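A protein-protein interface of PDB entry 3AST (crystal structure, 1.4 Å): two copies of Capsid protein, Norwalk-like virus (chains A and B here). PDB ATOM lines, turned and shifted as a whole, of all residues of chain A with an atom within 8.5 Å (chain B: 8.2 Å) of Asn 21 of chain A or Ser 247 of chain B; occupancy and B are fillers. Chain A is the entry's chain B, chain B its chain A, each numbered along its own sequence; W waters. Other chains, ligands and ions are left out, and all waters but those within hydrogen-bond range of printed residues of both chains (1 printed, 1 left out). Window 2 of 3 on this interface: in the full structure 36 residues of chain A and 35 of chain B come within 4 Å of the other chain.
Of the printed residues of chain B, Pro 20 of chain A touches Ser 247 (3.7 Å).
Of the printed residues of chain B, Asn 21 of chain A touches Ser 247 (2.8 Å).
Leu 24 of chain A touches none of the printed residues of chain B.
Gly 60 of chain B touches none of the printed residues of chain A.
Of the printed residues of chain A, Thr 243 of chain B touches Ile 22 (3.4 Å).
Ser 247 of chain B touches two residues of chain A.
The nearest printed residue of chain A that does not touch Thr 243 of chain B is Glu 240 of chain A (4.1 Å).
Printed residues of chain A that touch a printed residue of chain B: Pro 20, Asn 21, Ile 22 and Thr 26.
Of the 18 printed residues of chain B, 3 touch a printed residue of chain A.
Among the printed residues, 4 pairs touch across the chains.
Among the printed residues, no Asp or Glu carboxylate lies within 4 Å of a Lys or Arg side-chain nitrogen of the other chain.
Ser 247 of chain B touches Pro 20 of chain A.
Ile 22 of chain A touches Thr 243 of chain B.
CB of Ala 68 of chain B touches CG2 of Thr 26 of chain A, at 3.95 Å.
Positions printed for both chains: 240, 241 and 244.
Water W1 lies within hydrogen-bond range of a ring nitrogen (ND1) of His 244 of chain B (2.9 Å) and a ring nitrogen (ND1) of His 244 of chain A (3.2 Å).
The side-chain hydroxyl (OG1) of Thr 243 of chain B sits at hydrogen-bond distance from the backbone carbonyl oxygen (O) of Ala 68 of chain B (2.7 Å).
The side-chain hydroxyl (OG) of Ser 247 of chain B sits at hydrogen-bond distance from the backbone NH (N) of Asn 21 of chain A, 2.8 Å away.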
ATOM      1  N   THR A  18      -0.621  -3.285  27.822  1.00  0.00           N
ATOM      2  CA  THR A  18      -0.913  -1.849  27.836  1.00  0.00           C
ATOM      3  C   THR A  18      -0.809  -1.283  26.423  1.00  0.00           C
ATOM      4  O   THR A  18      -0.186  -1.886  25.546  1.00  0.00           O
ATOM      5  CB  THR A  18       0.087  -1.052  28.716  1.00  0.00           C
ATOM      6  OG1 THR A  18       1.425  -1.294  28.263  1.00  0.00           O
ATOM      7  CG2 THR A  18      -0.026  -1.432  30.192  1.00  0.00           C
ATOM      8  N   VAL A  19      -1.425  -0.124  26.210  1.00  0.00           N
ATOM      9  CA  VAL A  19      -1.181   0.663  24.999  1.00  0.00           C
ATOM     10  C   VAL A  19      -0.596   2.026  25.405  1.00  0.00           C
ATOM     11  O   VAL A  19      -0.803   2.466  26.539  1.00  0.00           O
ATOM     12  CB  VAL A  19      -2.453   0.817  24.115  1.00  0.00           C
ATOM     13  CG1 VAL A  19      -2.923  -0.543  23.608  1.00  0.00           C
ATOM     14  CG2 VAL A  19      -3.571   1.532  24.858  1.00  0.00           C
ATOM     15  N   PRO A  20       0.157   2.685  24.499  1.00  0.00           N
ATOM     16  CA  PRO A  20       0.777   3.977  24.817  1.00  0.00           C
ATOM     17  C   PRO A  20      -0.205   5.034  25.319  1.00  0.00           C
ATOM     18  O   PRO A  20      -1.321   5.143  24.809  1.00  0.00           O
ATOM     19  CB  PRO A  20       1.377   4.410  23.478  1.00  0.00           C
ATOM     20  CG  PRO A  20       1.711   3.135  22.810  1.00  0.00           C
ATOM     21  CD  PRO A  20       0.595   2.192  23.177  1.00  0.00           C
ATOM     22  N   ASN A  21       0.235   5.797  26.315  1.00  0.00           N
ATOM     23  CA  ASN A  21      -0.547   6.870  26.922  1.00  0.00           C
ATOM     24  C   ASN A  21      -0.246   8.193  26.219  1.00  0.00           C
ATOM     25  O   ASN A  21       0.356   9.105  26.792  1.00  0.00           O
ATOM     26  CB  ASN A  21      -0.239   6.945  28.427  1.00  0.00           C
ATOM     27  CG  ASN A  21      -1.182   7.870  29.189  1.00  0.00           C
ATOM     28  OD1 ASN A  21      -2.223   8.282  28.684  1.00  0.00           O
ATOM     29  ND2 ASN A  21      -0.815   8.191  30.426  1.00  0.00           N
ATOM     30  N   ILE A  22      -0.647   8.271  24.953  1.00  0.00           N
ATOM     31  CA  ILE A  22      -0.392   9.439  24.113  1.00  0.00           C
ATOM     32  C   ILE A  22      -1.640   9.708  23.270  1.00  0.00           C
ATOM     33  O   ILE A  22      -2.220   8.769  22.717  1.00  0.00           O
ATOM     34  CB  ILE A  22       0.857   9.229  23.205  1.00  0.00           C
ATOM     35  CG1 ILE A  22       2.129   9.151  24.062  1.00  0.00           C
ATOM     36  CG2 ILE A  22       0.988  10.350  22.165  1.00  0.00           C
ATOM     37  CD1 ILE A  22       3.368   8.748  23.314  1.00  0.00           C
ATOM     38  N   PRO A  23      -2.070  10.985  23.183  1.00  0.00           N
ATOM     39  CA  PRO A  23      -3.245  11.332  22.381  1.00  0.00           C
ATOM     40  C   PRO A  23      -3.123  10.911  20.918  1.00  0.00           C
ATOM     41  O   PRO A  23      -2.040  10.989  20.334  1.00  0.00           O
ATOM     42  CB  PRO A  23      -3.308  12.858  22.497  1.00  0.00           C
ATOM     43  CG  PRO A  23      -2.674  13.149  23.810  1.00  0.00           C
ATOM     44  CD  PRO A  23      -1.562  12.149  23.937  1.00  0.00           C
ATOM     45  N   LEU A  24      -4.235  10.471  20.342  1.00  0.00           N
ATOM     46  CA  LEU A  24      -4.247   9.940  18.980  1.00  0.00           C
ATOM     47  C   LEU A  24      -3.660  10.896  17.938  1.00  0.00           C
ATOM     48  O   LEU A  24      -2.899  10.471  17.062  1.00  0.00           O
ATOM     49  CB  LEU A  24      -5.666   9.522  18.591  1.00  0.00           C
ATOM     50  CG  LEU A  24      -5.868   8.857  17.228  1.00  0.00           C
ATOM     51  CD1 LEU A  24      -4.986   7.629  17.055  1.00  0.00           C
ATOM     52  CD2 LEU A  24      -7.323   8.491  17.056  1.00  0.00           C
ATOM     53  N   THR A  26      -1.362  12.852  18.151  1.00  0.00           N
ATOM     54  CA  THR A  26       0.085  12.975  18.313  1.00  0.00           C
ATOM     55  C   THR A  26       0.793  11.703  17.826  1.00  0.00           C
ATOM     56  O   THR A  26       2.016  11.678  17.675  1.00  0.00           O
ATOM     57  CB  THR A  26       0.424  13.313  19.785  1.00  0.00           C
ATOM     58  OG1 THR A  26      -0.258  14.521  20.149  1.00  0.00           O
ATOM     59  CG2 THR A  26       1.918  13.517  19.991  1.00  0.00           C
ATOM     60  N   LEU A  27       0.013  10.663  17.545  1.00  0.00           N
ATOM     61  CA  LEU A  27       0.553   9.387  17.069  1.00  0.00           C
ATOM     62  C   LEU A  27       0.734   9.371  15.556  1.00  0.00           C
ATOM     63  O   LEU A  27       0.209  10.235  14.854  1.00  0.00           O
ATOM     64  CB  LEU A  27      -0.349   8.235  17.517  1.00  0.00           C
ATOM     65  CG  LEU A  27      -0.457   8.035  19.032  1.00  0.00           C
ATOM     66  CD1 LEU A  27      -1.524   7.005  19.351  1.00  0.00           C
ATOM     67  CD2 LEU A  27       0.889   7.635  19.634  1.00  0.00           C
ATOM     68  N   GLU A 240       3.479   3.890  16.863  1.00  0.00           N
ATOM     69  CA  GLU A 240       3.910   3.844  18.262  1.00  0.00           C
ATOM     70  C   GLU A 240       3.339   2.646  19.012  1.00  0.00           C
ATOM     71  O   GLU A 240       3.963   2.149  19.943  1.00  0.00           O
ATOM     72  CB  GLU A 240       3.557   5.137  19.001  1.00  0.00           C
ATOM     73  CG  GLU A 240       4.335   6.366  18.539  1.00  0.00           C
ATOM     74  CD  GLU A 240       3.782   6.996  17.266  1.00  0.00           C
ATOM     75  OE1 GLU A 240       2.725   6.556  16.769  1.00  0.00           O
ATOM     76  OE2 GLU A 240       4.421   7.943  16.765  1.00  0.00           O
ATOM     77  N   TYR A 241       2.152   2.190  18.615  1.00  0.00           N
ATOM     78  CA  TYR A 241       1.586   0.969  19.192  1.00  0.00           C
ATOM     79  C   TYR A 241       2.447  -0.232  18.832  1.00  0.00           C
ATOM     80  O   TYR A 241       2.736  -1.076  19.680  1.00  0.00           O
ATOM     81  CB  TYR A 241       0.145   0.743  18.722  1.00  0.00           C
ATOM     82  CG  TYR A 241      -0.894   1.559  19.463  1.00  0.00           C
ATOM     83  CD1 TYR A 241      -2.126   1.003  19.803  1.00  0.00           C
ATOM     84  CD2 TYR A 241      -0.649   2.887  19.824  1.00  0.00           C
ATOM     85  CE1 TYR A 241      -3.085   1.753  20.484  1.00  0.00           C
ATOM     86  CE2 TYR A 241      -1.599   3.640  20.503  1.00  0.00           C
ATOM     87  CZ  TYR A 241      -2.809   3.068  20.825  1.00  0.00           C
ATOM     88  OH  TYR A 241      -3.740   3.828  21.497  1.00  0.00           O
ATOM     89  N   HIS A 244       5.636  -0.193  20.783  1.00  0.00           N
ATOM     90  CA  HIS A 244       5.293  -0.567  22.148  1.00  0.00           C
ATOM     91  C   HIS A 244       5.124  -2.078  22.286  1.00  0.00           C
ATOM     92  O   HIS A 244       5.676  -2.682  23.205  1.00  0.00           O
ATOM     93  CB  HIS A 244       4.023   0.167  22.580  1.00  0.00           C
ATOM     94  CG  HIS A 244       3.672  -0.016  24.023  1.00  0.00           C
ATOM     95  ND1 HIS A 244       4.411   0.542  25.045  1.00  0.00           N
ATOM     96  CD2 HIS A 244       2.645  -0.672  24.613  1.00  0.00           C
ATOM     97  CE1 HIS A 244       3.857   0.232  26.204  1.00  0.00           C
ATOM     98  NE2 HIS A 244       2.785  -0.504  25.971  1.00  0.00           N
ATOM     99  N   VAL A 262     -10.523   7.640  25.786  1.00  0.00           N
ATOM    100  CA  VAL A 262     -10.787   8.555  26.902  1.00  0.00           C
ATOM    101  C   VAL A 262     -10.329   9.982  26.600  1.00  0.00           C
ATOM    102  O   VAL A 262      -9.250  10.192  26.051  1.00  0.00           O
ATOM    103  CB  VAL A 262     -10.109   8.046  28.209  1.00  0.00           C
ATOM    104  CG1 VAL A 262     -10.455   8.938  29.395  1.00  0.00           C
ATOM    105  CG2 VAL A 262     -10.521   6.605  28.512  1.00  0.00           C
ATOM    106  N   PRO A 264      -8.579  12.964  27.859  1.00  0.00           N
ATOM    107  CA  PRO A 264      -7.641  13.134  28.976  1.00  0.00           C
ATOM    108  C   PRO A 264      -7.941  14.356  29.847  1.00  0.00           C
ATOM    109  O   PRO A 264      -7.575  14.374  31.024  1.00  0.00           O
ATOM    110  CB  PRO A 264      -6.282  13.283  28.281  1.00  0.00           C
ATOM    111  CG  PRO A 264      -6.595  13.749  26.914  1.00  0.00           C
ATOM    112  CD  PRO A 264      -7.920  13.153  26.553  1.00  0.00           C
ATOM    113  N   ASN A 267     -11.391  12.854  31.677  1.00  0.00           N
ATOM    114  CA  ASN A 267     -11.436  11.416  32.000  1.00  0.00           C
ATOM    115  C   ASN A 267     -12.727  10.701  31.573  1.00  0.00           C
ATOM    116  O   ASN A 267     -13.017   9.592  32.032  1.00  0.00           O
ATOM    117  CB  ASN A 267     -11.097  11.145  33.477  1.00  0.00           C
ATOM    118  CG  ASN A 267      -9.601  11.007  33.724  1.00  0.00           C
ATOM    119  OD1 ASN A 267      -8.789  11.101  32.800  1.00  0.00           O
ATOM    120  ND2 ASN A 267      -9.231  10.775  34.978  1.00  0.00           N
ATOM    121  N   GLY A 299      -8.140  12.183  22.085  1.00  0.00           N
ATOM    122  CA  GLY A 299      -8.362  11.122  23.064  1.00  0.00           C
ATOM    123  C   GLY A 299      -7.198  10.151  23.185  1.00  0.00           C
ATOM    124  O   GLY A 299      -6.327  10.088  22.312  1.00  0.00           O
ATOM    125  N   VAL A 300      -7.191   9.397  24.279  1.00  0.00           N
ATOM    126  CA  VAL A 300      -6.166   8.391  24.543  1.00  0.00           C
ATOM    127  C   VAL A 300      -6.856   7.040  24.717  1.00  0.00           C
ATOM    128  O   VAL A 300      -7.811   6.926  25.491  1.00  0.00           O
ATOM    129  CB  VAL A 300      -5.354   8.735  25.823  1.00  0.00           C
ATOM    130  CG1 VAL A 300      -4.319   7.653  26.125  1.00  0.00           C
ATOM    131  CG2 VAL A 300      -4.674  10.091  25.691  1.00  0.00           C
ATOM    132  N   PHE A 301      -6.389   6.022  23.994  1.00  0.00           N
ATOM    133  CA  PHE A 301      -6.912   4.675  24.195  1.00  0.00           C
ATOM    134  C   PHE A 301      -6.332   4.091  25.472  1.00  0.00           C
ATOM    135  O   PHE A 301      -5.148   4.268  25.770  1.00  0.00           O
ATOM    136  CB  PHE A 301      -6.602   3.753  23.013  1.00  0.00           C
ATOM    137  CG  PHE A 301      -7.373   4.070  21.761  1.00  0.00           C
ATOM    138  CD1 PHE A 301      -8.666   3.582  21.576  1.00  0.00           C
ATOM    139  CD2 PHE A 301      -6.795   4.835  20.751  1.00  0.00           C
ATOM    140  CE1 PHE A 301      -9.374   3.866  20.408  1.00  0.00           C
ATOM    141  CE2 PHE A 301      -7.497   5.124  19.585  1.00  0.00           C
ATOM    142  CZ  PHE A 301      -8.784   4.635  19.410  1.00  0.00           C
ATOM    143  N   LEU A 302      -7.181   3.407  26.227  1.00  0.00           N
ATOM    144  CA  LEU A 302      -6.793   2.801  27.493  1.00  0.00           C
ATOM    145  C   LEU A 302      -7.255   1.350  27.526  1.00  0.00           C
ATOM    146  O   LEU A 302      -8.423   1.060  27.279  1.00  0.00           O
ATOM    147  CB  LEU A 302      -7.417   3.583  28.656  1.00  0.00           C
ATOM    148  CG  LEU A 302      -7.226   3.063  30.084  1.00  0.00           C
ATOM    149  CD1 LEU A 302      -5.795   3.272  30.572  1.00  0.00           C
ATOM    150  CD2 LEU A 302      -8.223   3.726  31.029  1.00  0.00           C
ATOM    151  N   GLN B  12       0.664   5.531  39.674  1.00  0.00           N
ATOM    152  CA  GLN B  12       1.357   6.587  38.930  1.00  0.00           C
ATOM    153  C   GLN B  12       2.614   7.073  39.650  1.00  0.00           C
ATOM    154  O   GLN B  12       3.660   7.258  39.024  1.00  0.00           O
ATOM    155  CB  GLN B  12       0.423   7.771  38.669  1.00  0.00           C
ATOM    156  CG  GLN B  12      -0.625   7.530  37.590  1.00  0.00           C
ATOM    157  CD  GLN B  12      -1.658   8.641  37.522  1.00  0.00           C
ATOM    158  OE1 GLN B  12      -2.836   8.427  37.815  1.00  0.00           O
ATOM    159  NE2 GLN B  12      -1.222   9.838  37.140  1.00  0.00           N
ATOM    160  N   ARG B  15       5.277   4.133  39.738  1.00  0.00           N
ATOM    161  CA  ARG B  15       5.568   3.494  38.454  1.00  0.00           C
ATOM    162  C   ARG B  15       7.071   3.351  38.229  1.00  0.00           C
ATOM    163  O   ARG B  15       7.805   4.341  38.225  1.00  0.00           O
ATOM    164  CB  ARG B  15       4.926   4.270  37.302  1.00  0.00           C
ATOM    165  CG  ARG B  15       5.022   3.565  35.953  1.00  0.00           C
ATOM    166  CD  ARG B  15       4.198   4.275  34.893  1.00  0.00           C
ATOM    167  NE  ARG B  15       2.762   4.148  35.138  1.00  0.00           N
ATOM    168  CZ  ARG B  15       1.824   4.854  34.512  1.00  0.00           C
ATOM    169  NH1 ARG B  15       2.156   5.750  33.590  1.00  0.00           N
ATOM    170  NH2 ARG B  15       0.547   4.662  34.809  1.00  0.00           N
ATOM    171  N   CYS B  56      14.283  15.894  26.395  1.00  0.00           N
ATOM    172  CA  CYS B  56      13.205  15.416  27.247  1.00  0.00           C
ATOM    173  C   CYS B  56      13.788  14.945  28.564  1.00  0.00           C
ATOM    174  O   CYS B  56      14.766  14.194  28.584  1.00  0.00           O
ATOM    175  CB  CYS B  56      12.465  14.261  26.560  1.00  0.00           C
ATOM    176  SG  CYS B  56      10.923  13.770  27.365  1.00  0.00           S
ATOM    177  N   ASP B  59      11.507  11.829  33.211  1.00  0.00           N
ATOM    178  CA  ASP B  59      10.150  11.674  33.738  1.00  0.00           C
ATOM    179  C   ASP B  59       9.071  12.108  32.732  1.00  0.00           C
ATOM    180  O   ASP B  59       7.884  12.138  33.061  1.00  0.00           O
ATOM    181  CB  ASP B  59       9.992  12.392  35.092  1.00  0.00           C
ATOM    182  CG  ASP B  59      10.009  13.911  34.979  1.00  0.00           C
ATOM    183  OD1 ASP B  59      10.180  14.463  33.871  1.00  0.00           O
ATOM    184  OD2 ASP B  59       9.839  14.568  36.033  1.00  0.00           O
ATOM    185  N   GLY B  60       9.488  12.446  31.513  1.00  0.00           N
ATOM    186  CA  GLY B  60       8.553  12.722  30.419  1.00  0.00           C
ATOM    187  C   GLY B  60       8.241  14.173  30.101  1.00  0.00           C
ATOM    188  O   GLY B  60       7.295  14.452  29.364  1.00  0.00           O
ATOM    189  N   GLN B  61       9.038  15.097  30.630  1.00  0.00           N
ATOM    190  CA  GLN B  61       8.847  16.522  30.368  1.00  0.00           C
ATOM    191  C   GLN B  61       9.630  16.958  29.131  1.00  0.00           C
ATOM    192  O   GLN B  61      10.858  16.952  29.134  1.00  0.00           O
ATOM    193  CB  GLN B  61       9.263  17.348  31.593  1.00  0.00           C
ATOM    194  CG  GLN B  61       9.195  18.869  31.412  1.00  0.00           C
ATOM    195  CD  GLN B  61       7.786  19.382  31.181  1.00  0.00           C
ATOM    196  OE1 GLN B  61       6.919  19.268  32.049  1.00  0.00           O
ATOM    197  NE2 GLN B  61       7.553  19.961  30.008  1.00  0.00           N
ATOM    198  N   ALA B  68       6.664  14.919  21.008  1.00  0.00           N
ATOM    199  CA  ALA B  68       6.523  13.657  21.730  1.00  0.00           C
ATOM    200  C   ALA B  68       6.833  12.458  20.839  1.00  0.00           C
ATOM    201  O   ALA B  68       7.275  11.416  21.323  1.00  0.00           O
ATOM    202  CB  ALA B  68       5.118  13.537  22.311  1.00  0.00           C
ATOM    203  N   GLU B 240      12.531   7.156  20.338  1.00  0.00           N
ATOM    204  CA  GLU B 240      11.709   6.163  21.035  1.00  0.00           C
ATOM    205  C   GLU B 240      11.802   6.282  22.557  1.00  0.00           C
ATOM    206  O   GLU B 240      10.833   6.003  23.259  1.00  0.00           O
ATOM    207  CB  GLU B 240      12.053   4.739  20.590  1.00  0.00           C
ATOM    208  CG  GLU B 240      11.658   4.420  19.145  1.00  0.00           C
ATOM    209  CD  GLU B 240      12.641   4.948  18.105  1.00  0.00           C
ATOM    210  OE1 GLU B 240      13.709   5.483  18.472  1.00  0.00           O
ATOM    211  OE2 GLU B 240      12.337   4.828  16.900  1.00  0.00           O
ATOM    212  N   TYR B 241      12.969   6.691  23.056  1.00  0.00           N
ATOM    213  CA  TYR B 241      13.145   6.970  24.484  1.00  0.00           C
ATOM    214  C   TYR B 241      12.238   8.117  24.910  1.00  0.00           C
ATOM    215  O   TYR B 241      11.538   8.024  25.914  1.00  0.00           O
ATOM    216  CB  TYR B 241      14.600   7.323  24.784  1.00  0.00           C
ATOM    217  CG  TYR B 241      15.474   6.150  25.156  1.00  0.00           C
ATOM    218  CD1 TYR B 241      16.255   6.194  26.307  1.00  0.00           C
ATOM    219  CD2 TYR B 241      15.513   4.997  24.373  1.00  0.00           C
ATOM    220  CE1 TYR B 241      17.063   5.129  26.670  1.00  0.00           C
ATOM    221  CE2 TYR B 241      16.321   3.915  24.732  1.00  0.00           C
ATOM    222  CZ  TYR B 241      17.090   3.998  25.883  1.00  0.00           C
ATOM    223  OH  TYR B 241      17.891   2.945  26.261  1.00  0.00           O
ATOM    224  N   ILE B 242      12.242   9.192  24.127  1.00  0.00           N
ATOM    225  CA  ILE B 242      11.398  10.354  24.396  1.00  0.00           C
ATOM    226  C   ILE B 242       9.914   9.970  24.441  1.00  0.00           C
ATOM    227  O   ILE B 242       9.210  10.285  25.404  1.00  0.00           O
ATOM    228  CB  ILE B 242      11.666  11.476  23.367  1.00  0.00           C
ATOM    229  CG1 ILE B 242      13.110  11.966  23.515  1.00  0.00           C
ATOM    230  CG2 ILE B 242      10.658  12.620  23.528  1.00  0.00           C
ATOM    231  CD1 ILE B 242      13.587  12.873  22.395  1.00  0.00           C
ATOM    232  N   THR B 243       9.448   9.268  23.412  1.00  0.00           N
ATOM    233  CA  THR B 243       8.053   8.832  23.357  1.00  0.00           C
ATOM    234  C   THR B 243       7.713   7.958  24.567  1.00  0.00           C
ATOM    235  O   THR B 243       6.660   8.122  25.192  1.00  0.00           O
ATOM    236  CB  THR B 243       7.762   8.083  22.048  1.00  0.00           C
ATOM    237  OG1 THR B 243       8.160   8.903  20.943  1.00  0.00           O
ATOM    238  CG2 THR B 243       6.283   7.752  21.919  1.00  0.00           C
ATOM    239  N   HIS B 244       8.624   7.054  24.905  1.00  0.00           N
ATOM    240  CA  HIS B 244       8.449   6.175  26.050  1.00  0.00           C
ATOM    241  C   HIS B 244       8.307   6.966  27.350  1.00  0.00           C
ATOM    242  O   HIS B 244       7.381   6.712  28.127  1.00  0.00           O
ATOM    243  CB  HIS B 244       9.608   5.182  26.128  1.00  0.00           C
ATOM    244  CG  HIS B 244       9.426   4.113  27.159  1.00  0.00           C
ATOM    245  ND1 HIS B 244       8.474   3.122  27.044  1.00  0.00           N
ATOM    246  CD2 HIS B 244      10.079   3.876  28.321  1.00  0.00           C
ATOM    247  CE1 HIS B 244       8.553   2.318  28.090  1.00  0.00           C
ATOM    248  NE2 HIS B 244       9.518   2.754  28.880  1.00  0.00           N
ATOM    249  N   PHE B 245       9.193   7.935  27.570  1.00  0.00           N
ATOM    250  CA  PHE B 245       9.137   8.739  28.798  1.00  0.00           C
ATOM    251  C   PHE B 245       7.873   9.594  28.864  1.00  0.00           C
ATOM    252  O   PHE B 245       7.266   9.721  29.928  1.00  0.00           O
ATOM    253  CB  PHE B 245      10.383   9.615  28.967  1.00  0.00           C
ATOM    254  CG  PHE B 245      11.685   8.850  28.976  1.00  0.00           C
ATOM    255  CD1 PHE B 245      11.750   7.534  29.437  1.00  0.00           C
ATOM    256  CD2 PHE B 245      12.851   9.461  28.535  1.00  0.00           C
ATOM    257  CE1 PHE B 245      12.957   6.837  29.440  1.00  0.00           C
ATOM    258  CE2 PHE B 245      14.064   8.774  28.539  1.00  0.00           C
ATOM    259  CZ  PHE B 245      14.114   7.461  28.994  1.00  0.00           C
ATOM    260  N   VAL B 246       7.468  10.172  27.735  1.00  0.00           N
ATOM    261  CA  VAL B 246       6.235  10.966  27.682  1.00  0.00           C
ATOM    262  C   VAL B 246       5.025  10.099  28.048  1.00  0.00           C
ATOM    263  O   VAL B 246       4.157  10.527  28.814  1.00  0.00           O
ATOM    264  CB  VAL B 246       6.050  11.650  26.300  1.00  0.00           C
ATOM    265  CG1 VAL B 246       4.649  12.264  26.148  1.00  0.00           C
ATOM    266  CG2 VAL B 246       7.112  12.719  26.097  1.00  0.00           C
ATOM    267  N   SER B 247       4.986   8.877  27.524  1.00  0.00           N
ATOM    268  CA  SER B 247       3.905   7.940  27.826  1.00  0.00           C
ATOM    269  C   SER B 247       3.919   7.446  29.277  1.00  0.00           C
ATOM    270  O   SER B 247       2.883   7.452  29.949  1.00  0.00           O
ATOM    271  CB  SER B 247       3.945   6.756  26.857  1.00  0.00           C
ATOM    272  OG  SER B 247       2.919   5.824  27.148  1.00  0.00           O
ATOM    273  N   GLU B 248       5.091   7.031  29.752  1.00  0.00           N
ATOM    274  CA  GLU B 248       5.227   6.419  31.077  1.00  0.00           C
ATOM    275  C   GLU B 248       5.146   7.415  32.230  1.00  0.00           C
ATOM    276  O   GLU B 248       4.507   7.137  33.243  1.00  0.00           O
ATOM    277  CB  GLU B 248       6.537   5.631  31.179  1.00  0.00           C
ATOM    278  CG  GLU B 248       6.594   4.378  30.314  1.00  0.00           C
ATOM    279  CD  GLU B 248       5.745   3.249  30.858  1.00  0.00           C
ATOM    280  OE1 GLU B 248       5.877   2.922  32.055  1.00  0.00           O
ATOM    281  OE2 GLU B 248       4.950   2.682  30.080  1.00  0.00           O
ATOM    282  N   GLN B 249       5.812   8.559  32.083  1.00  0.00           N
ATOM    283  CA  GLN B 249       5.921   9.555  33.159  1.00  0.00           C
ATOM    284  C   GLN B 249       6.336   8.913  34.484  1.00  0.00           C
ATOM    285  O   GLN B 249       5.764   9.209  35.537  1.00  0.00           O
ATOM    286  CB  GLN B 249       4.614  10.343  33.332  1.00  0.00           C
ATOM    287  CG  GLN B 249       4.136  11.078  32.090  1.00  0.00           C
ATOM    288  CD  GLN B 249       2.818  11.804  32.308  1.00  0.00           C
ATOM    289  OE1 GLN B 249       2.723  13.010  32.085  1.00  0.00           O
ATOM    290  NE2 GLN B 249       1.797  11.075  32.754  1.00  0.00           N
ATOM    291  N   ALA B 250       7.321   8.023  34.425  1.00  0.00           N
ATOM    292  CA  ALA B 250       7.816   7.366  35.627  1.00  0.00           C
ATOM    293  C   ALA B 250       8.598   8.374  36.465  1.00  0.00           C
ATOM    294  O   ALA B 250       9.445   9.091  35.930  1.00  0.00           O
ATOM    295  CB  ALA B 250       8.685   6.179  35.269  1.00  0.00           C
HETATM  296  O   HOH W   1       5.826   3.290  25.812  1.00  0.00           O
